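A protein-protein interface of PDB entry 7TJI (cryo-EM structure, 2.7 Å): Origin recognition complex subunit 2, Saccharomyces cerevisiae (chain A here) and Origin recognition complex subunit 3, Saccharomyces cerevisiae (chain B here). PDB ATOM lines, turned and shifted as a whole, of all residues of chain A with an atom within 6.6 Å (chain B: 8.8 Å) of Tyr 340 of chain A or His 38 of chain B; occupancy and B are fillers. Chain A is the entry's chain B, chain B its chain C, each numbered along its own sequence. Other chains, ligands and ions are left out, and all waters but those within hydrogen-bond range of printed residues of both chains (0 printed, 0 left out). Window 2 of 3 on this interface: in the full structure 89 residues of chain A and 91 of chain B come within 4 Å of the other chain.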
ATOM      1  N   TRP A 305       3.493 -29.348  16.134  1.00  0.00           N
ATOM      2  CA  TRP A 305       2.547 -28.269  15.857  1.00  0.00           C
ATOM      3  C   TRP A 305       1.608 -28.041  17.040  1.00  0.00           C
ATOM      4  O   TRP A 305       1.343 -26.892  17.412  1.00  0.00           O
ATOM      5  CB  TRP A 305       1.789 -28.602  14.565  1.00  0.00           C
ATOM      6  CG  TRP A 305       0.651 -27.697  14.147  1.00  0.00           C
ATOM      7  CD1 TRP A 305       0.461 -26.387  14.478  1.00  0.00           C
ATOM      8  CD2 TRP A 305      -0.436 -28.049  13.285  1.00  0.00           C
ATOM      9  NE1 TRP A 305      -0.688 -25.913  13.902  1.00  0.00           N
ATOM     10  CE2 TRP A 305      -1.255 -26.913  13.159  1.00  0.00           C
ATOM     11  CE3 TRP A 305      -0.798 -29.220  12.611  1.00  0.00           C
ATOM     12  CZ2 TRP A 305      -2.414 -26.914  12.388  1.00  0.00           C
ATOM     13  CZ3 TRP A 305      -1.949 -29.218  11.852  1.00  0.00           C
ATOM     14  CH2 TRP A 305      -2.743 -28.075  11.744  1.00  0.00           C
ATOM     15  N   SER A 335       4.231 -23.592   8.677  1.00  0.00           N
ATOM     16  CA  SER A 335       3.717 -22.304   8.205  1.00  0.00           C
ATOM     17  C   SER A 335       2.390 -22.378   7.441  1.00  0.00           C
ATOM     18  O   SER A 335       1.456 -21.653   7.834  1.00  0.00           O
ATOM     19  CB  SER A 335       4.805 -21.600   7.383  1.00  0.00           C
ATOM     20  OG  SER A 335       4.320 -20.406   6.796  1.00  0.00           O
ATOM     21  N   PRO A 336       2.200 -23.214   6.396  1.00  0.00           N
ATOM     22  CA  PRO A 336       0.888 -23.184   5.729  1.00  0.00           C
ATOM     23  C   PRO A 336      -0.220 -23.835   6.532  1.00  0.00           C
ATOM     24  O   PRO A 336      -1.374 -23.420   6.400  1.00  0.00           O
ATOM     25  CB  PRO A 336       1.131 -23.910   4.398  1.00  0.00           C
ATOM     26  CG  PRO A 336       2.474 -24.483   4.461  1.00  0.00           C
ATOM     27  CD  PRO A 336       3.030 -24.293   5.815  1.00  0.00           C
ATOM     28  N   LYS A 337       0.088 -24.806   7.392  1.00  0.00           N
ATOM     29  CA  LYS A 337      -0.957 -25.379   8.233  1.00  0.00           C
ATOM     30  C   LYS A 337      -1.383 -24.427   9.344  1.00  0.00           C
ATOM     31  O   LYS A 337      -2.566 -24.393   9.701  1.00  0.00           O
ATOM     32  CB  LYS A 337      -0.498 -26.721   8.791  1.00  0.00           C
ATOM     33  CG  LYS A 337      -0.964 -27.863   7.917  1.00  0.00           C
ATOM     34  CD  LYS A 337      -0.550 -29.206   8.430  1.00  0.00           C
ATOM     35  CE  LYS A 337       0.189 -29.943   7.338  1.00  0.00           C
ATOM     36  NZ  LYS A 337      -0.221 -31.370   7.253  1.00  0.00           N
ATOM     37  N   ILE A 338      -0.453 -23.628   9.874  1.00  0.00           N
ATOM     38  CA  ILE A 338      -0.821 -22.571  10.812  1.00  0.00           C
ATOM     39  C   ILE A 338      -1.659 -21.507  10.112  1.00  0.00           C
ATOM     40  O   ILE A 338      -2.681 -21.050  10.647  1.00  0.00           O
ATOM     41  CB  ILE A 338       0.448 -21.988  11.471  1.00  0.00           C
ATOM     42  CG1 ILE A 338       0.849 -22.829  12.685  1.00  0.00           C
ATOM     43  CG2 ILE A 338       0.273 -20.525  11.867  1.00  0.00           C
ATOM     44  CD1 ILE A 338       2.022 -22.270  13.464  1.00  0.00           C
ATOM     45  N   ALA A 339      -1.270 -21.133   8.885  1.00  0.00           N
ATOM     46  CA  ALA A 339      -2.032 -20.148   8.121  1.00  0.00           C
ATOM     47  C   ALA A 339      -3.427 -20.654   7.757  1.00  0.00           C
ATOM     48  O   ALA A 339      -4.379 -19.868   7.727  1.00  0.00           O
ATOM     49  CB  ALA A 339      -1.262 -19.757   6.860  1.00  0.00           C
ATOM     50  N   TYR A 340      -3.567 -21.952   7.492  1.00  0.00           N
ATOM     51  CA  TYR A 340      -4.882 -22.508   7.204  1.00  0.00           C
ATOM     52  C   TYR A 340      -5.741 -22.607   8.458  1.00  0.00           C
ATOM     53  O   TYR A 340      -6.922 -22.248   8.426  1.00  0.00           O
ATOM     54  CB  TYR A 340      -4.738 -23.876   6.540  1.00  0.00           C
ATOM     55  CG  TYR A 340      -4.315 -23.801   5.090  1.00  0.00           C
ATOM     56  CD1 TYR A 340      -4.697 -22.731   4.292  1.00  0.00           C
ATOM     57  CD2 TYR A 340      -3.537 -24.803   4.518  1.00  0.00           C
ATOM     58  CE1 TYR A 340      -4.313 -22.656   2.965  1.00  0.00           C
ATOM     59  CE2 TYR A 340      -3.146 -24.738   3.196  1.00  0.00           C
ATOM     60  CZ  TYR A 340      -3.539 -23.663   2.423  1.00  0.00           C
ATOM     61  OH  TYR A 340      -3.154 -23.596   1.104  1.00  0.00           O
ATOM     62  N   SER A 341      -5.168 -23.079   9.571  1.00  0.00           N
ATOM     63  CA  SER A 341      -5.920 -23.213  10.812  1.00  0.00           C
ATOM     64  C   SER A 341      -6.308 -21.869  11.413  1.00  0.00           C
ATOM     65  O   SER A 341      -7.285 -21.802  12.164  1.00  0.00           O
ATOM     66  CB  SER A 341      -5.113 -24.015  11.832  1.00  0.00           C
ATOM     67  OG  SER A 341      -3.880 -23.378  12.125  1.00  0.00           O
ATOM     68  N   GLN A 342      -5.570 -20.806  11.105  1.00  0.00           N
ATOM     69  CA  GLN A 342      -5.912 -19.475  11.586  1.00  0.00           C
ATOM     70  C   GLN A 342      -6.805 -18.704  10.621  1.00  0.00           C
ATOM     71  O   GLN A 342      -7.189 -17.572  10.928  1.00  0.00           O
ATOM     72  CB  GLN A 342      -4.637 -18.677  11.868  1.00  0.00           C
ATOM     73  CG  GLN A 342      -3.907 -19.143  13.112  1.00  0.00           C
ATOM     74  CD  GLN A 342      -2.483 -18.644  13.187  1.00  0.00           C
ATOM     75  OE1 GLN A 342      -1.717 -19.062  14.054  1.00  0.00           O
ATOM     76  NE2 GLN A 342      -2.117 -17.743  12.285  1.00  0.00           N
ATOM     77  N   LEU A 343      -7.147 -19.286   9.478  1.00  0.00           N
ATOM     78  CA  LEU A 343      -8.007 -18.633   8.498  1.00  0.00           C
ATOM     79  C   LEU A 343      -9.460 -18.616   8.957  1.00  0.00           C
ATOM     80  O   LEU A 343     -10.124 -17.582   8.908  1.00  0.00           O
ATOM     81  CB  LEU A 343      -7.893 -19.332   7.143  1.00  0.00           C
ATOM     82  CG  LEU A 343      -8.689 -18.749   5.977  1.00  0.00           C
ATOM     83  CD1 LEU A 343      -8.292 -17.304   5.722  1.00  0.00           C
ATOM     84  CD2 LEU A 343      -8.485 -19.596   4.731  1.00  0.00           C
ATOM     85  N   SER A 357       0.973 -16.817   3.718  1.00  0.00           N
ATOM     86  CA  SER A 357       1.228 -17.746   4.815  1.00  0.00           C
ATOM     87  C   SER A 357       1.786 -17.011   6.037  1.00  0.00           C
ATOM     88  O   SER A 357       1.294 -15.949   6.407  1.00  0.00           O
ATOM     89  CB  SER A 357       2.188 -18.849   4.366  1.00  0.00           C
ATOM     90  OG  SER A 357       2.094 -19.980   5.210  1.00  0.00           O
ATOM     91  N   SER B  28       5.290 -20.853   0.098  1.00  0.00           N
ATOM     92  CA  SER B  28       4.079 -21.125  -0.655  1.00  0.00           C
ATOM     93  C   SER B  28       3.028 -21.778   0.240  1.00  0.00           C
ATOM     94  O   SER B  28       3.333 -22.364   1.281  1.00  0.00           O
ATOM     95  CB  SER B  28       4.389 -22.026  -1.850  1.00  0.00           C
ATOM     96  OG  SER B  28       5.210 -21.355  -2.790  1.00  0.00           O
ATOM     97  N   LEU B  29       1.773 -21.672  -0.183  1.00  0.00           N
ATOM     98  CA  LEU B  29       0.662 -22.233   0.576  1.00  0.00           C
ATOM     99  C   LEU B  29      -0.500 -22.593  -0.342  1.00  0.00           C
ATOM    100  O   LEU B  29      -0.299 -23.171  -1.409  1.00  0.00           O
ATOM    101  CB  LEU B  29       0.193 -21.257   1.662  1.00  0.00           C
ATOM    102  CG  LEU B  29      -0.535 -19.975   1.253  1.00  0.00           C
ATOM    103  CD1 LEU B  29      -1.539 -19.582   2.318  1.00  0.00           C
ATOM    104  CD2 LEU B  29       0.438 -18.837   1.013  1.00  0.00           C
ATOM    105  N   HIS B  38      -7.432 -29.569   9.677  1.00  0.00           N
ATOM    106  CA  HIS B  38      -7.044 -28.226  10.086  1.00  0.00           C
ATOM    107  C   HIS B  38      -6.646 -28.184  11.556  1.00  0.00           C
ATOM    108  O   HIS B  38      -6.397 -27.115  12.110  1.00  0.00           O
ATOM    109  CB  HIS B  38      -8.183 -27.240   9.823  1.00  0.00           C
ATOM    110  CG  HIS B  38      -8.029 -26.471   8.549  1.00  0.00           C
ATOM    111  ND1 HIS B  38      -8.512 -25.190   8.388  1.00  0.00           N
ATOM    112  CD2 HIS B  38      -7.440 -26.801   7.375  1.00  0.00           C
ATOM    113  CE1 HIS B  38      -8.233 -24.768   7.168  1.00  0.00           C
ATOM    114  NE2 HIS B  38      -7.581 -25.726   6.534  1.00  0.00           N
ATOM    115  N   ILE B  39      -6.598 -29.351  12.193  1.00  0.00           N
ATOM    116  CA  ILE B  39      -6.206 -29.448  13.596  1.00  0.00           C
ATOM    117  C   ILE B  39      -5.018 -30.400  13.704  1.00  0.00           C
ATOM    118  O   ILE B  39      -4.869 -31.299  12.864  1.00  0.00           O
ATOM    119  CB  ILE B  39      -7.383 -29.899  14.482  1.00  0.00           C
ATOM    120  CG1 ILE B  39      -7.905 -31.272  14.066  1.00  0.00           C
ATOM    121  CG2 ILE B  39      -8.509 -28.877  14.461  1.00  0.00           C
ATOM    122  CD1 ILE B  39      -8.915 -31.834  15.027  1.00  0.00           C
ATOM    123  N   PRO B  40      -4.130 -30.229  14.688  1.00  0.00           N
ATOM    124  CA  PRO B  40      -2.993 -31.153  14.824  1.00  0.00           C
ATOM    125  C   PRO B  40      -3.350 -32.519  15.387  1.00  0.00           C
ATOM    126  O   PRO B  40      -2.472 -33.387  15.434  1.00  0.00           O
ATOM    127  CB  PRO B  40      -2.045 -30.403  15.775  1.00  0.00           C
ATOM    128  CG  PRO B  40      -2.896 -29.435  16.488  1.00  0.00           C
ATOM    129  CD  PRO B  40      -3.953 -29.025  15.516  1.00  0.00           C
ATOM    130  N   PHE B  41      -4.588 -32.743  15.821  1.00  0.00           N
ATOM    131  CA  PHE B  41      -4.968 -34.028  16.394  1.00  0.00           C
ATOM    132  C   PHE B  41      -5.075 -35.095  15.309  1.00  0.00           C
ATOM    133  O   PHE B  41      -5.702 -34.878  14.268  1.00  0.00           O
ATOM    134  CB  PHE B  41      -6.290 -33.894  17.149  1.00  0.00           C
ATOM    135  CG  PHE B  41      -6.134 -33.521  18.599  1.00  0.00           C
ATOM    136  CD1 PHE B  41      -4.939 -33.003  19.076  1.00  0.00           C
ATOM    137  CD2 PHE B  41      -7.184 -33.693  19.484  1.00  0.00           C
ATOM    138  CE1 PHE B  41      -4.797 -32.664  20.404  1.00  0.00           C
ATOM    139  CE2 PHE B  41      -7.048 -33.355  20.818  1.00  0.00           C
ATOM    140  CZ  PHE B  41      -5.855 -32.840  21.277  1.00  0.00           C
ATOM    141  N   GLU B  51     -13.563 -39.258  12.172  1.00  0.00           N
ATOM    142  CA  GLU B  51     -13.071 -37.893  12.034  1.00  0.00           C
ATOM    143  C   GLU B  51     -13.743 -36.956  13.030  1.00  0.00           C
ATOM    144  O   GLU B  51     -13.094 -36.040  13.554  1.00  0.00           O
ATOM    145  CB  GLU B  51     -13.283 -37.402  10.599  1.00  0.00           C
ATOM    146  CG  GLU B  51     -12.923 -35.936  10.302  1.00  0.00           C
ATOM    147  CD  GLU B  51     -11.423 -35.643  10.159  1.00  0.00           C
ATOM    148  OE1 GLU B  51     -10.584 -36.179  10.918  1.00  0.00           O
ATOM    149  OE2 GLU B  51     -11.082 -34.847   9.260  1.00  0.00           O
ATOM    150  N   VAL B  54     -12.143 -37.121  16.470  1.00  0.00           N
ATOM    151  CA  VAL B  54     -10.929 -36.314  16.543  1.00  0.00           C
ATOM    152  C   VAL B  54     -11.268 -34.854  16.830  1.00  0.00           C
ATOM    153  O   VAL B  54     -10.661 -34.215  17.701  1.00  0.00           O
ATOM    154  CB  VAL B  54     -10.132 -36.470  15.236  1.00  0.00           C
ATOM    155  CG1 VAL B  54      -8.925 -35.567  15.219  1.00  0.00           C
ATOM    156  CG2 VAL B  54      -9.715 -37.917  15.041  1.00  0.00           C
ATOM    157  N   GLU B  55     -12.261 -34.317  16.116  1.00  0.00           N
ATOM    158  CA  GLU B  55     -12.689 -32.937  16.325  1.00  0.00           C
ATOM    159  C   GLU B  55     -13.295 -32.745  17.709  1.00  0.00           C
ATOM    160  O   GLU B  55     -13.050 -31.728  18.370  1.00  0.00           O
ATOM    161  CB  GLU B  55     -13.692 -32.538  15.244  1.00  0.00           C
ATOM    162  CG  GLU B  55     -13.686 -31.065  14.894  1.00  0.00           C
ATOM    163  CD  GLU B  55     -12.797 -30.752  13.709  1.00  0.00           C
ATOM    164  OE1 GLU B  55     -13.225 -30.994  12.561  1.00  0.00           O
ATOM    165  OE2 GLU B  55     -11.670 -30.261  13.926  1.00  0.00           O
ATOM    166  N   TRP B  58     -10.600 -32.557  20.161  1.00  0.00           N
ATOM    167  CA  TRP B  58      -9.970 -31.238  20.090  1.00  0.00           C
ATOM    168  C   TRP B  58     -10.762 -30.200  20.878  1.00  0.00           C
ATOM    169  O   TRP B  58     -10.194 -29.426  21.661  1.00  0.00           O
ATOM    170  CB  TRP B  58      -9.824 -30.821  18.627  1.00  0.00           C
ATOM    171  CG  TRP B  58      -9.264 -29.456  18.421  1.00  0.00           C
ATOM    172  CD1 TRP B  58      -9.930 -28.362  17.978  1.00  0.00           C
ATOM    173  CD2 TRP B  58      -7.912 -29.041  18.642  1.00  0.00           C
ATOM    174  NE1 TRP B  58      -9.086 -27.283  17.915  1.00  0.00           N
ATOM    175  CE2 TRP B  58      -7.838 -27.675  18.317  1.00  0.00           C
ATOM    176  CE3 TRP B  58      -6.759 -29.693  19.086  1.00  0.00           C
ATOM    177  CZ2 TRP B  58      -6.657 -26.950  18.415  1.00  0.00           C
ATOM    178  CZ3 TRP B  58      -5.589 -28.973  19.186  1.00  0.00           C
ATOM    179  CH2 TRP B  58      -5.546 -27.614  18.854  1.00  0.00           C
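OG of Ser 335 of chain A is in hydrogen-bond range of OG of Ser 357 of chain A (2.8 Å).
The side-chain hydroxyl (OG) of Ser 341 of chain A is in hydrogen-bond range of the backbone carbonyl oxygen (O) of Lys 337 of chain A.
OG of Ser 341 of chain A lies within hydrogen-bond range of O of Ile 338 of chain A.
Of the printed residues of chain B, Trp 305 of chain A touches His 38, Ile 39 and Pro 40.
Of the printed residues of chain B, Pro 336 of chain A touches Ser 28 (3.9 Å) and Leu 29 (3.9 Å).
No residue of chain B comes within 4 Å of Ala 339 of chain A.
Of chain B, only Leu 29 and His 38 come within 4 Å of Tyr 340 of chain A.
Ser 341 of chain A touches just one residue of chain B: His 38.
Of the printed residues of chain A, His 38 of chain B touches Trp 305 (3.8 Å), Tyr 340 (3.1 Å) and Ser 341 (3.4 Å).
Trp 58 of chain B touches none of the printed residues of chain A.
The nearest printed residue of chain A that does not touch Pro 40 of chain B is Ser 341 of chain A (6.3 Å).
Hydrophobic or aromatic side chains of chain B within 4 Å of the printed part of chain A: Leu 29, His 38 and Pro 40.
Among the printed residues, 9 pairs touch across the chains.
Among the printed residues, no Asp or Glu carboxylate lies within 4 Å of a Lys or Arg side-chain nitrogen of the other chain.
A ring nitrogen (ND1) of His 38 of chain B sits close to the backbone carbonyl oxygen of Tyr 340 of chain A, at 3.3 Å.
Among the printed residues, merely in contact across the chains: Trp 305 of chain A with His 38 of chain B (3.8 Å), Trp 305 of chain A with Ile 39 of chain B (3.7 Å), Trp 305 of chain A with Pro 40 of chain B (3.6 Å), Pro 336 of chain A with Ser 28 of chain B (3.9 Å), Pro 336 of chain A with Leu 29 of chain B (3.9 Å), Tyr 340 of chain A with Leu 29 of chain B (3.2 Å), Ser 341 of chain A with His 38 of chain B (3.4 Å) and Ser 357 of chain A with Leu 29 of chain B (3.4 Å).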
